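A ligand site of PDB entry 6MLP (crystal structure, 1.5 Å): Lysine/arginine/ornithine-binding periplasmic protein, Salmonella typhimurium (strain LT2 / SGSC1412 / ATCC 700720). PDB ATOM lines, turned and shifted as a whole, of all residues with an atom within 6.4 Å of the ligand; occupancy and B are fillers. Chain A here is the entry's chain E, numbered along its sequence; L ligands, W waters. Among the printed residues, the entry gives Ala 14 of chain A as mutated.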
ATOM      1  N   ASP A  11       0.362   3.017  -6.401  1.00  0.00           N
ATOM      2  CA  ASP A  11       0.191   4.024  -5.347  1.00  0.00           C
ATOM      3  C   ASP A  11      -1.167   3.781  -4.692  1.00  0.00           C
ATOM      4  O   ASP A  11      -2.211   4.044  -5.282  1.00  0.00           O
ATOM      5  CB  ASP A  11       0.292   5.419  -5.970  1.00  0.00           C
ATOM      6  CG  ASP A  11      -0.218   6.534  -5.063  1.00  0.00           C
ATOM      7  OD1 ASP A  11      -0.457   6.330  -3.849  1.00  0.00           O
ATOM      8  OD2 ASP A  11      -0.380   7.658  -5.589  1.00  0.00           O
ATOM      9  N   THR A  13      -3.105   5.215  -2.637  1.00  0.00           N
ATOM     10  CA  THR A  13      -3.867   6.349  -2.099  1.00  0.00           C
ATOM     11  C   THR A  13      -4.885   6.860  -3.128  1.00  0.00           C
ATOM     12  O   THR A  13      -5.214   8.055  -3.178  1.00  0.00           O
ATOM     13  CB  THR A  13      -2.943   7.499  -1.586  1.00  0.00           C
ATOM     14  OG1 THR A  13      -2.162   8.047  -2.661  1.00  0.00           O
ATOM     15  CG2 THR A  13      -2.007   6.977  -0.505  1.00  0.00           C
ATOM     16  N   ALA A  14      -5.412   5.936  -3.927  1.00  0.00           N
ATOM     17  CA  ALA A  14      -6.366   6.278  -4.985  1.00  0.00           C
ATOM     18  C   ALA A  14      -7.597   5.376  -4.987  1.00  0.00           C
ATOM     19  O   ALA A  14      -7.912   4.744  -6.010  1.00  0.00           O
ATOM     20  CB  ALA A  14      -5.667   6.261  -6.366  1.00  0.00           C
ATOM     21  N   PHE A  52       3.671   7.529  -5.875  1.00  0.00           N
ATOM     22  CA  PHE A  52       3.405   7.617  -7.304  1.00  0.00           C
ATOM     23  C   PHE A  52       4.616   8.093  -8.109  1.00  0.00           C
ATOM     24  O   PHE A  52       4.919   7.542  -9.179  1.00  0.00           O
ATOM     25  CB  PHE A  52       2.218   8.548  -7.573  1.00  0.00           C
ATOM     26  CG  PHE A  52       1.778   8.529  -9.002  1.00  0.00           C
ATOM     27  CD1 PHE A  52       0.987   7.488  -9.466  1.00  0.00           C
ATOM     28  CD2 PHE A  52       2.175   9.528  -9.873  1.00  0.00           C
ATOM     29  CE1 PHE A  52       0.581   7.451 -10.789  1.00  0.00           C
ATOM     30  CE2 PHE A  52       1.776   9.502 -11.191  1.00  0.00           C
ATOM     31  CZ  PHE A  52       0.973   8.468 -11.653  1.00  0.00           C
ATOM     32  N   SER A  69      -1.756   1.788 -11.640  1.00  0.00           N
ATOM     33  CA  SER A  69      -1.901   2.826 -10.645  1.00  0.00           C
ATOM     34  C   SER A  69      -2.631   4.018 -11.276  1.00  0.00           C
ATOM     35  O   SER A  69      -2.197   5.142 -11.145  1.00  0.00           O
ATOM     36  CB  SER A  69      -0.506   3.257 -10.175  1.00  0.00           C
ATOM     37  OG  SER A  69      -0.570   3.939  -8.937  1.00  0.00           O
ATOM     38  N   SER A  70      -3.755   3.732 -11.948  1.00  0.00           N
ATOM     39  CA  SER A  70      -4.470   4.763 -12.729  1.00  0.00           C
ATOM     40  C   SER A  70      -3.492   5.548 -13.598  1.00  0.00           C
ATOM     41  O   SER A  70      -3.580   6.773 -13.683  1.00  0.00           O
ATOM     42  CB  SER A  70      -5.241   5.735 -11.824  1.00  0.00           C
ATOM     43  OG  SER A  70      -6.166   5.063 -10.979  1.00  0.00           O
ATOM     44  N   LEU A  71      -2.556   4.846 -14.232  1.00  0.00           N
ATOM     45  CA  LEU A  71      -1.474   5.520 -14.927  1.00  0.00           C
ATOM     46  C   LEU A  71      -1.929   5.989 -16.310  1.00  0.00           C
ATOM     47  O   LEU A  71      -2.082   5.189 -17.231  1.00  0.00           O
ATOM     48  CB  LEU A  71      -0.255   4.608 -15.038  1.00  0.00           C
ATOM     49  CG  LEU A  71       1.009   5.273 -15.596  1.00  0.00           C
ATOM     50  CD1 LEU A  71       1.578   6.210 -14.559  1.00  0.00           C
ATOM     51  CD2 LEU A  71       2.032   4.202 -16.002  1.00  0.00           C
ATOM     52  N   SER A  72      -2.164   7.292 -16.424  1.00  0.00           N
ATOM     53  CA  SER A  72      -2.655   7.859 -17.684  1.00  0.00           C
ATOM     54  C   SER A  72      -1.658   7.669 -18.807  1.00  0.00           C
ATOM     55  O   SER A  72      -0.454   7.861 -18.621  1.00  0.00           O
ATOM     56  CB  SER A  72      -2.954   9.349 -17.490  1.00  0.00           C
ATOM     57  OG  SER A  72      -4.044   9.525 -16.610  1.00  0.00           O
ATOM     58  N   ILE A  73      -2.200   7.301 -19.978  1.00  0.00           N
ATOM     59  CA  ILE A  73      -1.417   7.064 -21.178  1.00  0.00           C
ATOM     60  C   ILE A  73      -1.235   8.394 -21.918  1.00  0.00           C
ATOM     61  O   ILE A  73      -2.121   8.836 -22.655  1.00  0.00           O
ATOM     62  CB  ILE A  73      -2.138   6.054 -22.111  1.00  0.00           C
ATOM     63  CG1 ILE A  73      -2.520   4.773 -21.364  1.00  0.00           C
ATOM     64  CG2 ILE A  73      -1.260   5.743 -23.331  1.00  0.00           C
ATOM     65  CD1 ILE A  73      -3.428   3.865 -22.157  1.00  0.00           C
ATOM     66  N   THR A  74      -0.096   9.044 -21.703  1.00  0.00           N
ATOM     67  CA  THR A  74       0.177  10.347 -22.301  1.00  0.00           C
ATOM     68  C   THR A  74       1.314  10.267 -23.309  1.00  0.00           C
ATOM     69  O   THR A  74       2.153   9.379 -23.227  1.00  0.00           O
ATOM     70  CB  THR A  74       0.573  11.377 -21.236  1.00  0.00           C
ATOM     71  OG1 THR A  74       1.859  11.023 -20.709  1.00  0.00           O
ATOM     72  CG2 THR A  74      -0.453  11.414 -20.113  1.00  0.00           C
ATOM     73  N   ARG A  77       4.678  10.387 -21.519  1.00  0.00           N
ATOM     74  CA  ARG A  77       5.083   9.127 -20.911  1.00  0.00           C
ATOM     75  C   ARG A  77       5.457   8.068 -21.931  1.00  0.00           C
ATOM     76  O   ARG A  77       6.335   7.255 -21.661  1.00  0.00           O
ATOM     77  CB  ARG A  77       4.000   8.605 -19.969  1.00  0.00           C
ATOM     78  CG  ARG A  77       3.954   9.380 -18.669  1.00  0.00           C
ATOM     79  CD  ARG A  77       2.713   9.019 -17.897  1.00  0.00           C
ATOM     80  NE  ARG A  77       2.683   9.757 -16.631  1.00  0.00           N
ATOM     81  CZ  ARG A  77       1.626   9.819 -15.838  1.00  0.00           C
ATOM     82  NH1 ARG A  77       0.508   9.183 -16.164  1.00  0.00           N
ATOM     83  NH2 ARG A  77       1.687  10.497 -14.695  1.00  0.00           N
ATOM     84  N   ALA A  90     -10.048   8.276 -17.617  1.00  0.00           N
ATOM     85  CA  ALA A  90      -9.806   9.058 -16.400  1.00  0.00           C
ATOM     86  C   ALA A  90      -9.657  10.545 -16.698  1.00  0.00           C
ATOM     87  O   ALA A  90      -8.612  10.992 -17.175  1.00  0.00           O
ATOM     88  CB  ALA A  90      -8.571   8.556 -15.667  1.00  0.00           C
ATOM     89  N   SER A  92      -9.815  14.617 -15.170  1.00  0.00           N
ATOM     90  CA  SER A  92      -9.444  15.321 -13.937  1.00  0.00           C
ATOM     91  C   SER A  92     -10.493  16.335 -13.547  1.00  0.00           C
ATOM     92  O   SER A  92     -11.199  16.874 -14.398  1.00  0.00           O
ATOM     93  CB  SER A  92      -8.123  16.061 -14.143  1.00  0.00           C
ATOM     94  OG  SER A  92      -7.075  15.158 -14.444  1.00  0.00           O
ATOM     95  N   LEU A 117      -0.881  15.622  -6.825  1.00  0.00           N
ATOM     96  CA  LEU A 117       0.039  14.498  -6.579  1.00  0.00           C
ATOM     97  C   LEU A 117       1.358  14.676  -7.330  1.00  0.00           C
ATOM     98  O   LEU A 117       1.374  14.891  -8.544  1.00  0.00           O
ATOM     99  CB  LEU A 117      -0.651  13.190  -6.988  1.00  0.00           C
ATOM    100  CG  LEU A 117       0.117  11.876  -6.860  1.00  0.00           C
ATOM    101  CD1 LEU A 117       0.360  11.563  -5.384  1.00  0.00           C
ATOM    102  CD2 LEU A 117      -0.692  10.769  -7.516  1.00  0.00           C
ATOM    103  N   GLY A 119       4.357  14.015  -9.532  1.00  0.00           N
ATOM    104  CA  GLY A 119       4.573  13.065 -10.612  1.00  0.00           C
ATOM    105  C   GLY A 119       3.356  12.828 -11.493  1.00  0.00           C
ATOM    106  O   GLY A 119       3.450  12.124 -12.498  1.00  0.00           O
ATOM    107  N   SER A 120       2.227  13.429 -11.129  1.00  0.00           N
ATOM    108  CA  SER A 120       0.979  13.178 -11.845  1.00  0.00           C
ATOM    109  C   SER A 120       0.807  14.086 -13.048  1.00  0.00           C
ATOM    110  O   SER A 120       1.487  15.109 -13.191  1.00  0.00           O
ATOM    111  CB  SER A 120      -0.227  13.355 -10.914  1.00  0.00           C
ATOM    112  OG  SER A 120      -0.348  14.718 -10.533  1.00  0.00           O
ATOM    113  N   THR A 121      -0.121  13.708 -13.909  1.00  0.00           N
ATOM    114  CA  THR A 121      -0.512  14.570 -15.015  1.00  0.00           C
ATOM    115  C   THR A 121      -1.123  15.867 -14.468  1.00  0.00           C
ATOM    116  O   THR A 121      -0.968  16.921 -15.084  1.00  0.00           O
ATOM    117  CB  THR A 121      -1.542  13.887 -15.914  1.00  0.00           C
ATOM    118  OG1 THR A 121      -2.632  13.464 -15.095  1.00  0.00           O
ATOM    119  CG2 THR A 121      -0.931  12.657 -16.585  1.00  0.00           C
ATOM    120  N   GLN A 122      -1.831  15.789 -13.344  1.00  0.00           N
ATOM    121  CA  GLN A 122      -2.374  16.990 -12.721  1.00  0.00           C
ATOM    122  C   GLN A 122      -1.269  17.940 -12.268  1.00  0.00           C
ATOM    123  O   GLN A 122      -1.429  19.164 -12.406  1.00  0.00           O
ATOM    124  CB  GLN A 122      -3.288  16.649 -11.533  1.00  0.00           C
ATOM    125  CG  GLN A 122      -4.578  15.927 -11.946  1.00  0.00           C
ATOM    126  CD  GLN A 122      -4.420  14.432 -12.061  1.00  0.00           C
ATOM    127  OE1 GLN A 122      -3.419  13.850 -11.628  1.00  0.00           O
ATOM    128  NE2 GLN A 122      -5.430  13.776 -12.632  1.00  0.00           N
ATOM    129  N   GLN A 143      -1.791  11.014  -2.143  1.00  0.00           N
ATOM    130  CA  GLN A 143      -3.069  11.723  -2.187  1.00  0.00           C
ATOM    131  C   GLN A 143      -3.737  11.796  -0.812  1.00  0.00           C
ATOM    132  O   GLN A 143      -4.561  12.670  -0.551  1.00  0.00           O
ATOM    133  CB  GLN A 143      -3.983  11.091  -3.248  1.00  0.00           C
ATOM    134  CG  GLN A 143      -5.326  11.773  -3.452  1.00  0.00           C
ATOM    135  CD  GLN A 143      -5.276  12.999  -4.347  1.00  0.00           C
ATOM    136  OE1 GLN A 143      -4.464  13.079  -5.274  1.00  0.00           O
ATOM    137  NE2 GLN A 143      -6.154  13.965  -4.076  1.00  0.00           N
ATOM    138  N   GLN A 160      -7.203  16.155  -9.117  1.00  0.00           N
ATOM    139  CA  GLN A 160      -6.891  14.740  -9.203  1.00  0.00           C
ATOM    140  C   GLN A 160      -7.875  14.095 -10.169  1.00  0.00           C
ATOM    141  O   GLN A 160      -8.725  14.784 -10.736  1.00  0.00           O
ATOM    142  CB  GLN A 160      -6.973  14.057  -7.829  1.00  0.00           C
ATOM    143  CG  GLN A 160      -8.328  14.208  -7.155  1.00  0.00           C
ATOM    144  CD  GLN A 160      -8.494  15.585  -6.524  1.00  0.00           C
ATOM    145  OE1 GLN A 160      -7.654  16.011  -5.741  1.00  0.00           O
ATOM    146  NE2 GLN A 160      -9.556  16.295  -6.901  1.00  0.00           N
ATOM    147  N   ASP A 161      -7.785  12.781 -10.348  1.00  0.00           N
ATOM    148  CA  ASP A 161      -8.736  12.089 -11.220  1.00  0.00           C
ATOM    149  C   ASP A 161     -10.130  12.217 -10.635  1.00  0.00           C
ATOM    150  O   ASP A 161     -10.347  12.067  -9.429  1.00  0.00           O
ATOM    151  CB  ASP A 161      -8.400  10.604 -11.397  1.00  0.00           C
ATOM    152  CG  ASP A 161      -7.141  10.371 -12.225  1.00  0.00           C
ATOM    153  OD1 ASP A 161      -6.676  11.275 -12.964  1.00  0.00           O
ATOM    154  OD2 ASP A 161      -6.630   9.233 -12.153  1.00  0.00           O
ATOM    155  N   PHE A 191      -3.454  15.193 -20.233  1.00  0.00           N
ATOM    156  CA  PHE A 191      -4.162  14.184 -19.468  1.00  0.00           C
ATOM    157  C   PHE A 191      -4.222  12.818 -20.131  1.00  0.00           C
ATOM    158  O   PHE A 191      -4.603  11.822 -19.496  1.00  0.00           O
ATOM    159  CB  PHE A 191      -5.543  14.707 -19.068  1.00  0.00           C
ATOM    160  CG  PHE A 191      -5.478  15.882 -18.123  1.00  0.00           C
ATOM    161  CD1 PHE A 191      -4.764  15.799 -16.943  1.00  0.00           C
ATOM    162  CD2 PHE A 191      -6.096  17.080 -18.444  1.00  0.00           C
ATOM    163  CE1 PHE A 191      -4.682  16.876 -16.080  1.00  0.00           C
ATOM    164  CE2 PHE A 191      -6.026  18.164 -17.580  1.00  0.00           C
ATOM    165  CZ  PHE A 191      -5.318  18.058 -16.399  1.00  0.00           C
ATOM    166  N   THR A 195      -6.184   5.234 -18.866  1.00  0.00           N
ATOM    167  CA  THR A 195      -5.071   4.658 -18.123  1.00  0.00           C
ATOM    168  C   THR A 195      -4.682   3.304 -18.697  1.00  0.00           C
ATOM    169  O   THR A 195      -5.473   2.690 -19.410  1.00  0.00           O
ATOM    170  CB  THR A 195      -5.425   4.485 -16.638  1.00  0.00           C
ATOM    171  OG1 THR A 195      -6.415   3.446 -16.494  1.00  0.00           O
ATOM    172  CG2 THR A 195      -5.943   5.796 -16.054  1.00  0.00           C
HETATM  173  N1  LIG L   1      -4.126   9.422 -13.641  1.00  0.00           N
HETATM  174  C1  LIG L   1      -3.213  10.477 -13.179  1.00  0.00           C
HETATM  175  C2  LIG L   1      -1.791  10.179 -13.613  1.00  0.00           C
HETATM  176  O1  LIG L   1      -1.579   9.154 -14.290  1.00  0.00           O
HETATM  177  C3  LIG L   1      -3.327  10.737 -11.652  1.00  0.00           C
HETATM  178  C4  LIG L   1      -3.099   9.542 -10.766  1.00  0.00           C
HETATM  179  N2  LIG L   1      -3.280   9.600  -9.405  1.00  0.00           N
HETATM  180  C5  LIG L   1      -2.708   8.277 -11.042  1.00  0.00           C
HETATM  181  C6  LIG L   1      -3.015   8.425  -8.866  1.00  0.00           C
HETATM  182  N3  LIG L   1      -2.670   7.594  -9.839  1.00  0.00           N
HETATM  183  O2  LIG L   1      -0.869  10.956 -13.350  1.00  0.00           O
HETATM  184  O   HOH W   1      -3.557  12.671  -9.149  1.00  0.00           O
HETATM  185  O   HOH W   2      -5.856  11.149  -9.181  1.00  0.00           O
HETATM  186  O   HOH W   3      -4.278  10.710  -6.797  1.00  0.00           O
HETATM  187  O   HOH W   4      -2.693   5.187  -7.957  1.00  0.00           O
HETATM  188  O   HOH W   5      -2.873   8.716  -5.438  1.00  0.00           O
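O of Ser 70 sits at hydrogen-bond distance from N1 of the ligand (2.7 Å). OG of Ser 72 is in hydrogen-bond range of N1 of the ligand (3.0 Å). An oxygen (O1) of the ligand is in hydrogen-bond range of the backbone NH (N) of Ser 72, at 2.9 Å. An oxygen (O1) of the ligand is in salt-bridge range of the guanidinium group of Arg 77 (2.8 Å). An oxygen (O2) of the ligand is in hydrogen-bond range of the backbone NH (N) of Thr 121 (2.9 Å). N3 of the ligand is in hydrogen-bond range of O of Ser 69, 2.8 Å away. OD2 of Asp 161 is in salt-bridge range of N1 of the ligand (2.9 Å).
The side-chain amide nitrogen (NE2) of Gln 122 sits at hydrogen-bond distance from the side-chain hydroxyl (OG) of Ser 92 (2.8 Å). The backbone NH of Gln 122 sits close to the side-chain hydroxyl of Ser 120 (3.4 Å). The side-chain hydroxyl (OG) of Ser 69 lies within hydrogen-bond range of the backbone NH (N) of Asp 11, at 2.9 Å. OD1 of Asp 161 sits at hydrogen-bond distance from NE2 of Gln 122 (2.8 Å). The guanidinium group (NH1) of Arg 77 sits at hydrogen-bond distance from the backbone carbonyl oxygen (O) of Ser 72 (3.0 Å). OG1 of Thr 74 is in hydrogen-bond range of N of Arg 77, at 3.0 Å. The side-chain hydroxyl (OG) of Ser 120 lies within hydrogen-bond range of the backbone carbonyl oxygen (O) of Leu 117 (2.6 Å). The backbone carbonyl oxygen of Gly 119 lies within hydrogen-bond range of the guanidinium group of Arg 77, at 3.3 Å.
Phe 52 touches the ligand (CE1 to N3, 3.4 Å). Leu 71 touches the ligand (CA to O1, 3.7 Å). CD2 of Leu 117 touches N2 of the ligand, 3.4 Å away. Ser 120 touches the ligand. OE1 of Gln 122 touches C3 of the ligand (3.1 Å). Hydrophobic or aromatic side chains within 4 Å of the ligand: Phe 52 and Leu 117. 11 residues have an atom within 4 Å of the ligand: Phe 52, Ser 69, Ser 70, Leu 71, Ser 72, Arg 77, Leu 117, Ser 120, Thr 121, Gln 122 and Asp 161. The nearest printed residue that does not touch the ligand is Ala 14 (4.2 Å).
Water W3 lies within hydrogen-bond range of the side-chain amide oxygen of Gln 143 (2.8 Å) and a nitrogen (N2) of the ligand (3.0 Å). Water W2 bridges the backbone NH of Asp 161 (2.8 Å) and a nitrogen (N2) of the ligand (3.0 Å). Water W4 lies within hydrogen-bond range of OG of Ser 69, O of Asp 11 and N3 of the ligand. Water W1 lies within hydrogen-bond range of OE1 of Gln 122 (2.7 Å) and N2 of the ligand (3.1 Å). Water W5 bridges OD2 of Asp 11 and OG1 of Thr 13.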
